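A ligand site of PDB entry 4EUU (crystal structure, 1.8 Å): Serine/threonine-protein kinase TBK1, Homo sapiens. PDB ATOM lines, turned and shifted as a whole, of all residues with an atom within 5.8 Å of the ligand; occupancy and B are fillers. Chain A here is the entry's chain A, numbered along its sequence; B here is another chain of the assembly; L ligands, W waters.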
ATOM      1  N   LEU A  17     -24.126 -22.203  28.256  1.00  0.00           N
ATOM      2  CA  LEU A  17     -23.450 -21.060  27.597  1.00  0.00           C
ATOM      3  C   LEU A  17     -22.002 -20.914  28.043  1.00  0.00           C
ATOM      4  O   LEU A  17     -21.194 -20.276  27.351  1.00  0.00           O
ATOM      5  CB  LEU A  17     -24.196 -19.740  27.888  1.00  0.00           C
ATOM      6  CG  LEU A  17     -25.608 -19.682  27.290  1.00  0.00           C
ATOM      7  CD1 LEU A  17     -26.279 -18.353  27.706  1.00  0.00           C
ATOM      8  CD2 LEU A  17     -25.520 -19.817  25.731  1.00  0.00           C
ATOM      9  N   GLY A  18     -21.679 -21.441  29.212  1.00  0.00           N
ATOM     10  CA  GLY A  18     -20.323 -21.291  29.736  1.00  0.00           C
ATOM     11  C   GLY A  18     -20.068 -22.296  30.845  1.00  0.00           C
ATOM     12  O   GLY A  18     -20.979 -22.717  31.529  1.00  0.00           O
ATOM     13  N   GLN A  19     -18.815 -22.691  31.025  1.00  0.00           N
ATOM     14  CA  GLN A  19     -18.528 -23.773  32.025  1.00  0.00           C
ATOM     15  C   GLN A  19     -17.301 -23.295  32.801  1.00  0.00           C
ATOM     16  O   GLN A  19     -16.408 -22.707  32.209  1.00  0.00           O
ATOM     17  CB  GLN A  19     -18.394 -25.138  31.285  1.00  0.00           C
ATOM     18  CG  GLN A  19     -17.469 -26.292  31.886  1.00  0.00           C
ATOM     19  CD  GLN A  19     -17.250 -27.478  30.879  1.00  0.00           C
ATOM     20  OE1 GLN A  19     -18.066 -27.707  29.984  1.00  0.00           O
ATOM     21  NE2 GLN A  19     -16.163 -28.212  31.043  1.00  0.00           N
ATOM     22  N   GLY A  20     -17.281 -23.457  34.135  1.00  0.00           N
ATOM     23  CA  GLY A  20     -16.181 -22.876  34.900  1.00  0.00           C
ATOM     24  C   GLY A  20     -15.937 -23.647  36.181  1.00  0.00           C
ATOM     25  O   GLY A  20     -16.697 -24.579  36.471  1.00  0.00           O
ATOM     26  N   ALA A  21     -14.913 -23.225  36.949  1.00  0.00           N
ATOM     27  CA  ALA A  21     -14.539 -23.867  38.218  1.00  0.00           C
ATOM     28  C   ALA A  21     -15.627 -23.848  39.296  1.00  0.00           C
ATOM     29  O   ALA A  21     -15.794 -24.804  40.055  1.00  0.00           O
ATOM     30  CB  ALA A  21     -13.221 -23.230  38.782  1.00  0.00           C
ATOM     31  N   ALA A  23     -18.859 -22.419  38.677  1.00  0.00           N
ATOM     32  CA  ALA A  23     -20.199 -22.163  38.145  1.00  0.00           C
ATOM     33  C   ALA A  23     -20.350 -22.514  36.666  1.00  0.00           C
ATOM     34  O   ALA A  23     -19.355 -22.510  35.911  1.00  0.00           O
ATOM     35  CB  ALA A  23     -20.577 -20.684  38.376  1.00  0.00           C
ATOM     36  N   ASN A  24     -21.585 -22.806  36.230  1.00  0.00           N
ATOM     37  CA  ASN A  24     -21.913 -22.828  34.817  1.00  0.00           C
ATOM     38  C   ASN A  24     -22.881 -21.718  34.484  1.00  0.00           C
ATOM     39  O   ASN A  24     -23.567 -21.209  35.380  1.00  0.00           O
ATOM     40  CB  ASN A  24     -22.487 -24.184  34.418  1.00  0.00           C
ATOM     41  CG  ASN A  24     -21.493 -25.305  34.660  1.00  0.00           C
ATOM     42  OD1 ASN A  24     -20.329 -25.170  34.360  1.00  0.00           O
ATOM     43  ND2 ASN A  24     -21.971 -26.406  35.220  1.00  0.00           N
ATOM     44  N   VAL A  25     -22.900 -21.303  33.222  1.00  0.00           N
ATOM     45  CA  VAL A  25     -23.901 -20.324  32.772  1.00  0.00           C
ATOM     46  C   VAL A  25     -24.822 -21.038  31.795  1.00  0.00           C
ATOM     47  O   VAL A  25     -24.342 -21.790  30.923  1.00  0.00           O
ATOM     48  CB  VAL A  25     -23.297 -19.119  32.085  1.00  0.00           C
ATOM     49  CG1 VAL A  25     -24.431 -18.153  31.654  1.00  0.00           C
ATOM     50  CG2 VAL A  25     -22.354 -18.379  33.054  1.00  0.00           C
ATOM     51  N   ALA A  38     -29.153 -15.120  30.479  1.00  0.00           N
ATOM     52  CA  ALA A  38     -28.049 -15.997  30.840  1.00  0.00           C
ATOM     53  C   ALA A  38     -28.026 -16.149  32.345  1.00  0.00           C
ATOM     54  O   ALA A  38     -28.006 -15.153  33.085  1.00  0.00           O
ATOM     55  CB  ALA A  38     -26.707 -15.417  30.331  1.00  0.00           C
ATOM     56  N   LYS A  40     -26.361 -17.728  35.742  1.00  0.00           N
ATOM     57  CA  LYS A  40     -25.142 -18.284  36.297  1.00  0.00           C
ATOM     58  C   LYS A  40     -25.501 -19.025  37.583  1.00  0.00           C
ATOM     59  O   LYS A  40     -26.142 -18.469  38.481  1.00  0.00           O
ATOM     60  CB  LYS A  40     -24.085 -17.159  36.533  1.00  0.00           C
ATOM     61  CG  LYS A  40     -22.742 -17.702  37.093  1.00  0.00           C
ATOM     62  CD  LYS A  40     -21.639 -16.592  36.935  1.00  0.00           C
ATOM     63  CE  LYS A  40     -20.372 -17.000  37.599  1.00  0.00           C
ATOM     64  NZ  LYS A  40     -19.356 -15.927  37.315  1.00  0.00           N
ATOM     65  N   VAL A  70     -22.063  -6.480  30.974  1.00  0.00           N
ATOM     66  CA  VAL A  70     -23.265  -7.286  30.813  1.00  0.00           C
ATOM     67  C   VAL A  70     -24.187  -7.019  31.987  1.00  0.00           C
ATOM     68  O   VAL A  70     -23.763  -6.987  33.143  1.00  0.00           O
ATOM     69  CB  VAL A  70     -22.917  -8.799  30.663  1.00  0.00           C
ATOM     70  CG1 VAL A  70     -24.183  -9.671  30.758  1.00  0.00           C
ATOM     71  CG2 VAL A  70     -22.225  -9.043  29.324  1.00  0.00           C
ATOM     72  N   MET A  88     -28.744 -12.720  34.131  1.00  0.00           N
ATOM     73  CA  MET A  88     -28.059 -11.680  33.372  1.00  0.00           C
ATOM     74  C   MET A  88     -28.572 -11.544  31.959  1.00  0.00           C
ATOM     75  O   MET A  88     -29.266 -12.409  31.441  1.00  0.00           O
ATOM     76  CB  MET A  88     -26.521 -11.976  33.351  1.00  0.00           C
ATOM     77  CG  MET A  88     -25.856 -11.915  34.760  1.00  0.00           C
ATOM     78  SD  MET A  88     -24.140 -12.443  34.570  1.00  0.00           S
ATOM     79  CE  MET A  88     -24.367 -14.212  34.506  1.00  0.00           C
ATOM     80  N   GLU A  89     -28.234 -10.417  31.335  1.00  0.00           N
ATOM     81  CA  GLU A  89     -28.491 -10.216  29.938  1.00  0.00           C
ATOM     82  C   GLU A  89     -27.922 -11.372  29.103  1.00  0.00           C
ATOM     83  O   GLU A  89     -26.777 -11.800  29.311  1.00  0.00           O
ATOM     84  CB  GLU A  89     -27.829  -8.889  29.535  1.00  0.00           C
ATOM     85  CG  GLU A  89     -27.512  -8.761  28.114  1.00  0.00           C
ATOM     86  CD  GLU A  89     -26.836  -7.410  27.803  1.00  0.00           C
ATOM     87  OE1 GLU A  89     -26.303  -6.731  28.722  1.00  0.00           O
ATOM     88  OE2 GLU A  89     -26.847  -7.051  26.636  1.00  0.00           O
ATOM     89  N   PHE A  90     -28.747 -11.908  28.199  1.00  0.00           N
ATOM     90  CA  PHE A  90     -28.247 -12.897  27.212  1.00  0.00           C
ATOM     91  C   PHE A  90     -27.675 -12.203  25.971  1.00  0.00           C
ATOM     92  O   PHE A  90     -28.312 -11.332  25.433  1.00  0.00           O
ATOM     93  CB  PHE A  90     -29.359 -13.870  26.820  1.00  0.00           C
ATOM     94  CG  PHE A  90     -28.968 -14.853  25.742  1.00  0.00           C
ATOM     95  CD1 PHE A  90     -27.860 -15.665  25.884  1.00  0.00           C
ATOM     96  CD2 PHE A  90     -29.737 -14.974  24.574  1.00  0.00           C
ATOM     97  CE1 PHE A  90     -27.509 -16.577  24.894  1.00  0.00           C
ATOM     98  CE2 PHE A  90     -29.424 -15.898  23.596  1.00  0.00           C
ATOM     99  CZ  PHE A  90     -28.306 -16.718  23.751  1.00  0.00           C
ATOM    100  N   CYS A  91     -26.455 -12.566  25.563  1.00  0.00           N
ATOM    101  CA  CYS A  91     -25.816 -12.023  24.390  1.00  0.00           C
ATOM    102  C   CYS A  91     -25.733 -13.126  23.350  1.00  0.00           C
ATOM    103  O   CYS A  91     -24.785 -13.918  23.359  1.00  0.00           O
ATOM    104  CB  CYS A  91     -24.385 -11.515  24.737  1.00  0.00           C
ATOM    105  SG  CYS A  91     -24.368 -10.308  26.069  1.00  0.00           S
ATOM    106  N   PRO A  92     -26.717 -13.186  22.418  1.00  0.00           N
ATOM    107  CA  PRO A  92     -26.839 -14.296  21.486  1.00  0.00           C
ATOM    108  C   PRO A  92     -25.645 -14.456  20.557  1.00  0.00           C
ATOM    109  O   PRO A  92     -25.368 -15.593  20.102  1.00  0.00           O
ATOM    110  CB  PRO A  92     -28.120 -13.950  20.699  1.00  0.00           C
ATOM    111  CG  PRO A  92     -28.311 -12.500  20.894  1.00  0.00           C
ATOM    112  CD  PRO A  92     -27.854 -12.261  22.293  1.00  0.00           C
ATOM    113  N   CYS A  93     -24.929 -13.367  20.283  1.00  0.00           N
ATOM    114  CA  CYS A  93     -23.704 -13.424  19.448  1.00  0.00           C
ATOM    115  C   CYS A  93     -22.481 -14.072  20.098  1.00  0.00           C
ATOM    116  O   CYS A  93     -21.507 -14.311  19.404  1.00  0.00           O
ATOM    117  CB  CYS A  93     -23.284 -12.023  19.006  1.00  0.00           C
ATOM    118  SG  CYS A  93     -24.605 -11.275  18.018  1.00  0.00           S
ATOM    119  N   GLY A  94     -22.502 -14.275  21.421  1.00  0.00           N
ATOM    120  CA  GLY A  94     -21.358 -14.906  22.084  1.00  0.00           C
ATOM    121  C   GLY A  94     -20.173 -13.941  22.249  1.00  0.00           C
ATOM    122  O   GLY A  94     -20.373 -12.748  22.352  1.00  0.00           O
ATOM    123  N   SER A  95     -18.959 -14.483  22.298  1.00  0.00           N
ATOM    124  CA  SER A  95     -17.802 -13.735  22.784  1.00  0.00           C
ATOM    125  C   SER A  95     -16.807 -13.306  21.717  1.00  0.00           C
ATOM    126  O   SER A  95     -16.789 -13.791  20.599  1.00  0.00           O
ATOM    127  CB  SER A  95     -17.017 -14.578  23.796  1.00  0.00           C
ATOM    128  OG  SER A  95     -16.354 -15.653  23.123  1.00  0.00           O
ATOM    129  N   TYR A  97     -13.807 -14.118  21.903  1.00  0.00           N
ATOM    130  CA  TYR A  97     -13.028 -15.351  21.655  1.00  0.00           C
ATOM    131  C   TYR A  97     -13.508 -15.993  20.344  1.00  0.00           C
ATOM    132  O   TYR A  97     -12.715 -16.323  19.436  1.00  0.00           O
ATOM    133  CB  TYR A  97     -13.215 -16.343  22.823  1.00  0.00           C
ATOM    134  CG  TYR A  97     -12.756 -17.741  22.491  1.00  0.00           C
ATOM    135  CD1 TYR A  97     -11.436 -18.085  22.635  1.00  0.00           C
ATOM    136  CD2 TYR A  97     -13.657 -18.691  22.020  1.00  0.00           C
ATOM    137  CE1 TYR A  97     -11.004 -19.352  22.322  1.00  0.00           C
ATOM    138  CE2 TYR A  97     -13.227 -19.958  21.693  1.00  0.00           C
ATOM    139  CZ  TYR A  97     -11.897 -20.263  21.845  1.00  0.00           C
ATOM    140  OH  TYR A  97     -11.441 -21.511  21.558  1.00  0.00           O
ATOM    141  N   THR A  98     -14.828 -16.126  20.202  1.00  0.00           N
ATOM    142  CA  THR A  98     -15.363 -16.795  19.019  1.00  0.00           C
ATOM    143  C   THR A  98     -15.061 -16.012  17.737  1.00  0.00           C
ATOM    144  O   THR A  98     -14.738 -16.597  16.683  1.00  0.00           O
ATOM    145  CB  THR A  98     -16.870 -17.039  19.213  1.00  0.00           C
ATOM    146  OG1 THR A  98     -17.001 -17.873  20.353  1.00  0.00           O
ATOM    147  CG2 THR A  98     -17.484 -17.761  18.018  1.00  0.00           C
ATOM    148  N   GLY A 141     -12.688 -14.561  25.929  1.00  0.00           N
ATOM    149  CA  GLY A 141     -13.756 -15.482  26.343  1.00  0.00           C
ATOM    150  C   GLY A 141     -14.824 -14.864  27.236  1.00  0.00           C
ATOM    151  O   GLY A 141     -15.953 -15.356  27.297  1.00  0.00           O
ATOM    152  N   ASN A 142     -14.521 -13.776  27.932  1.00  0.00           N
ATOM    153  CA  ASN A 142     -15.578 -13.142  28.667  1.00  0.00           C
ATOM    154  C   ASN A 142     -15.807 -11.672  28.303  1.00  0.00           C
ATOM    155  O   ASN A 142     -16.302 -10.875  29.094  1.00  0.00           O
ATOM    156  CB  ASN A 142     -15.434 -13.414  30.170  1.00  0.00           C
ATOM    157  CG  ASN A 142     -14.117 -12.991  30.680  1.00  0.00           C
ATOM    158  OD1 ASN A 142     -13.566 -12.007  30.202  1.00  0.00           O
ATOM    159  ND2 ASN A 142     -13.572 -13.750  31.688  1.00  0.00           N
ATOM    160  N   MET A 144     -18.207  -9.974  25.845  1.00  0.00           N
ATOM    161  CA  MET A 144     -19.329 -10.428  25.004  1.00  0.00           C
ATOM    162  C   MET A 144     -19.642  -9.438  23.882  1.00  0.00           C
ATOM    163  O   MET A 144     -19.544  -8.229  24.092  1.00  0.00           O
ATOM    164  CB  MET A 144     -20.568 -10.626  25.842  1.00  0.00           C
ATOM    165  CG  MET A 144     -20.335 -11.527  27.046  1.00  0.00           C
ATOM    166  SD  MET A 144     -19.639 -13.150  26.595  1.00  0.00           S
ATOM    167  CE  MET A 144     -20.991 -13.882  25.752  1.00  0.00           C
ATOM    168  N   THR A 158     -17.912  -9.445  31.171  1.00  0.00           N
ATOM    169  CA  THR A 158     -18.676 -10.306  32.081  1.00  0.00           C
ATOM    170  C   THR A 158     -17.737 -11.245  32.799  1.00  0.00           C
ATOM    171  O   THR A 158     -16.525 -11.078  32.723  1.00  0.00           O
ATOM    172  CB  THR A 158     -19.821 -11.064  31.362  1.00  0.00           C
ATOM    173  OG1 THR A 158     -20.722 -11.625  32.337  1.00  0.00           O
ATOM    174  CG2 THR A 158     -19.282 -12.181  30.541  1.00  0.00           C
ATOM    175  N   ASP A 159     -18.287 -12.209  33.535  1.00  0.00           N
ATOM    176  CA  ASP A 159     -17.543 -13.112  34.413  1.00  0.00           C
ATOM    177  C   ASP A 159     -16.780 -12.418  35.513  1.00  0.00           C
ATOM    178  O   ASP A 159     -15.556 -12.288  35.469  1.00  0.00           O
ATOM    179  CB  ASP A 159     -16.611 -14.054  33.651  1.00  0.00           C
ATOM    180  CG  ASP A 159     -16.018 -15.114  34.564  1.00  0.00           C
ATOM    181  OD1 ASP A 159     -16.302 -15.098  35.759  1.00  0.00           O
ATOM    182  OD2 ASP A 159     -15.285 -15.977  34.100  1.00  0.00           O
ATOM    183  N   LEU B  13     -23.615 -22.121  17.226  1.00  0.00           N
ATOM    184  CA  LEU B  13     -22.474 -21.899  18.130  1.00  0.00           C
ATOM    185  C   LEU B  13     -22.918 -21.568  19.552  1.00  0.00           C
ATOM    186  O   LEU B  13     -22.113 -21.623  20.468  1.00  0.00           O
ATOM    187  CB  LEU B  13     -21.600 -20.756  17.570  1.00  0.00           C
ATOM    188  CG  LEU B  13     -21.082 -21.086  16.173  1.00  0.00           C
ATOM    189  CD1 LEU B  13     -20.405 -19.834  15.570  1.00  0.00           C
ATOM    190  CD2 LEU B  13     -20.118 -22.235  16.325  1.00  0.00           C
ATOM    191  N   SER B  14     -24.214 -21.274  19.759  1.00  0.00           N
ATOM    192  CA  SER B  14     -24.685 -21.066  21.129  1.00  0.00           C
ATOM    193  C   SER B  14     -25.165 -22.350  21.765  1.00  0.00           C
ATOM    194  O   SER B  14     -25.449 -22.370  22.987  1.00  0.00           O
ATOM    195  CB  SER B  14     -25.783 -20.018  21.184  1.00  0.00           C
ATOM    196  OG  SER B  14     -26.908 -20.398  20.398  1.00  0.00           O
ATOM    197  N   ILE B  16     -24.088 -25.076  23.237  1.00  0.00           N
ATOM    198  CA  ILE B  16     -22.911 -25.737  23.786  1.00  0.00           C
ATOM    199  C   ILE B  16     -23.281 -26.900  24.692  1.00  0.00           C
ATOM    200  O   ILE B  16     -24.259 -26.795  25.443  1.00  0.00           O
ATOM    201  CB  ILE B  16     -22.069 -24.702  24.535  1.00  0.00           C
ATOM    202  CG1 ILE B  16     -21.586 -23.683  23.483  1.00  0.00           C
ATOM    203  CG2 ILE B  16     -20.958 -25.392  25.299  1.00  0.00           C
ATOM    204  CD1 ILE B  16     -21.332 -22.325  23.993  1.00  0.00           C
ATOM    205  N   GLY B  18     -20.243 -28.763  26.073  1.00  0.00           N
ATOM    206  CA  GLY B  18     -19.030 -28.948  26.879  1.00  0.00           C
ATOM    207  C   GLY B  18     -17.940 -28.031  26.311  1.00  0.00           C
ATOM    208  O   GLY B  18     -17.961 -27.704  25.101  1.00  0.00           O
ATOM    209  N   GLN B  19     -17.024 -27.598  27.181  1.00  0.00           N
ATOM    210  CA  GLN B  19     -15.969 -26.574  26.839  1.00  0.00           C
ATOM    211  C   GLN B  19     -14.640 -27.136  27.350  1.00  0.00           C
ATOM    212  O   GLN B  19     -14.603 -27.757  28.412  1.00  0.00           O
ATOM    213  CB  GLN B  19     -16.371 -25.219  27.518  1.00  0.00           C
ATOM    214  CG  GLN B  19     -15.278 -24.102  27.698  1.00  0.00           C
ATOM    215  CD  GLN B  19     -15.700 -22.864  28.617  1.00  0.00           C
ATOM    216  OE1 GLN B  19     -16.894 -22.470  28.736  1.00  0.00           O
ATOM    217  NE2 GLN B  19     -14.689 -22.253  29.210  1.00  0.00           N
ATOM    218  N   ASN B  24     -14.579 -27.612  21.838  1.00  0.00           N
ATOM    219  CA  ASN B  24     -15.888 -27.513  22.473  1.00  0.00           C
ATOM    220  C   ASN B  24     -16.774 -28.547  21.838  1.00  0.00           C
ATOM    221  O   ASN B  24     -16.478 -29.016  20.737  1.00  0.00           O
ATOM    222  CB  ASN B  24     -16.475 -26.130  22.229  1.00  0.00           C
ATOM    223  CG  ASN B  24     -15.638 -25.043  22.853  1.00  0.00           C
ATOM    224  OD1 ASN B  24     -15.221 -25.179  23.987  1.00  0.00           O
ATOM    225  ND2 ASN B  24     -15.445 -23.964  22.133  1.00  0.00           N
HETATM  226  I1  LIG L   1     -23.369 -13.662  31.096  1.00  0.00           I
HETATM  227  S1  LIG L   1     -18.786 -17.571  34.255  1.00  0.00           S
HETATM  228  O1  LIG L   1     -19.388 -19.263  22.954  1.00  0.00           O
HETATM  229  O2  LIG L   1     -19.698 -15.840  31.866  1.00  0.00           O
HETATM  230  N1  LIG L   1     -18.565 -20.574  24.671  1.00  0.00           N
HETATM  231  N2  LIG L   1     -20.612 -19.265  24.895  1.00  0.00           N
HETATM  232  N3  LIG L   1     -21.848 -16.220  29.592  1.00  0.00           N
HETATM  233  N4  LIG L   1     -24.065 -15.835  25.294  1.00  0.00           N
HETATM  234  N5  LIG L   1     -18.458 -17.049  30.299  1.00  0.00           N
HETATM  235  N6  LIG L   1     -22.997 -16.023  27.460  1.00  0.00           N
HETATM  236  N7  LIG L   1     -24.557 -14.356  27.024  1.00  0.00           N
HETATM  237  C1  LIG L   1     -17.089 -22.270  24.746  1.00  0.00           C
HETATM  238  C2  LIG L   1     -17.862 -22.219  26.086  1.00  0.00           C
HETATM  239  C3  LIG L   1     -18.744 -20.978  25.992  1.00  0.00           C
HETATM  240  C4  LIG L   1     -17.442 -21.014  23.994  1.00  0.00           C
HETATM  241  C5  LIG L   1     -19.494 -19.682  24.084  1.00  0.00           C
HETATM  242  C6  LIG L   1     -21.660 -18.423  24.359  1.00  0.00           C
HETATM  243  C7  LIG L   1     -22.308 -17.524  25.163  1.00  0.00           C
HETATM  244  C8  LIG L   1     -19.842 -16.794  28.377  1.00  0.00           C
HETATM  245  C9  LIG L   1     -21.979 -18.630  23.027  1.00  0.00           C
HETATM  246  C10 LIG L   1     -21.079 -17.373  29.128  1.00  0.00           C
HETATM  247  C11 LIG L   1     -23.356 -16.791  24.585  1.00  0.00           C
HETATM  248  C12 LIG L   1     -18.860 -16.053  29.325  1.00  0.00           C
HETATM  249  C13 LIG L   1     -22.994 -17.867  22.475  1.00  0.00           C
HETATM  250  C14 LIG L   1     -23.675 -16.987  23.261  1.00  0.00           C
HETATM  251  C15 LIG L   1     -22.799 -15.551  28.688  1.00  0.00           C
HETATM  252  C16 LIG L   1     -23.865 -15.397  26.620  1.00  0.00           C
HETATM  253  C17 LIG L   1     -23.522 -14.428  29.179  1.00  0.00           C
HETATM  254  C18 LIG L   1     -18.987 -16.831  31.606  1.00  0.00           C
HETATM  255  C19 LIG L   1     -24.423 -13.817  28.244  1.00  0.00           C
HETATM  256  C20 LIG L   1     -18.705 -17.884  32.651  1.00  0.00           C
HETATM  257  C21 LIG L   1     -18.398 -19.258  32.343  1.00  0.00           C
HETATM  258  C22 LIG L   1     -18.241 -20.003  33.682  1.00  0.00           C
HETATM  259  C23 LIG L   1     -18.401 -19.084  34.773  1.00  0.00           C
HETATM  260  O   HOH W   1     -16.723 -20.396  37.337  1.00  0.00           O
HETATM  261  O   HOH W   2     -16.760 -18.227  23.899  1.00  0.00           O
HETATM  262  O   HOH W   3     -17.155 -19.357  28.955  1.00  0.00           O
HETATM  263  O   HOH W   4     -19.534 -20.828  20.691  1.00  0.00           O
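Merely in contact with the ligand: Gly 18 of chain A, Gln 19 of chain A, Gly 20, Ala 23, Val 25, Ala 38, Met 88, Glu 89, Phe 90, Pro 92, Gly 94, Thr 98, Gly 141, Met 144, Thr 158, Asp 159, Leu 13 of chain B, Ser 14 of chain B, Ile 16 of chain B, Gln 19 of chain B and Asn 24 of chain B.
Hydrophobic or aromatic side chains that line the ligand: Leu 17, Val 25, Ala 38, Met 88, Phe 90, Met 144 and Ile 16 of chain B.
Of the 32 residues printed, 24 come within 4 Å of the ligand.
The backbone NH (N) of Leu 17 lies within hydrogen-bond range of the backbone carbonyl oxygen (O) of Val 25.
N of Gln 19 of chain B lies within hydrogen-bond range of OE1 of Gln 19 of chain A (3.0 Å).
The backbone NH (N) of Met 88 lies within hydrogen-bond range of the backbone carbonyl oxygen (O) of Ala 38, at 2.7 Å.
The side-chain carboxylate (OD1) of Asp 159 is in salt-bridge range of the side-chain amino group (NZ) of Lys 40, at 3.5 Å.
The backbone NH (N) of Thr 158 is in hydrogen-bond range of the backbone carbonyl oxygen (O) of Asn 142.
O of Gly 18 of chain A is in hydrogen-bond range of N of Val 25, at 2.9 Å.
The side-chain hydroxyl of Ser 95 sits at hydrogen-bond distance from the backbone NH of Thr 98, 3.3 Å away.
O of Leu 17 lies within hydrogen-bond range of N2 of the ligand, at 2.7 Å.
The backbone NH (N) of Cys 91 lies within hydrogen-bond range of a nitrogen (N7) of the ligand.
The backbone carbonyl oxygen (O) of Cys 91 is in hydrogen-bond range of a nitrogen (N4) of the ligand, 2.8 Å away.
NZ of Lys 40 lies close to S1 of the ligand (3.5 Å).
Water W4 lies within hydrogen-bond range of O of Leu 13 of chain B and O1 of the ligand.
Water W2 bridges the side-chain hydroxyl (OG) of Ser 95 (2.7 Å) and an oxygen (O1) of the ligand (3.0 Å).
Water W3 lies within hydrogen-bond range of a nitrogen (N5) of the ligand (3.0 Å) and the side-chain amide oxygen of Gln 19 of chain B (3.1 Å).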
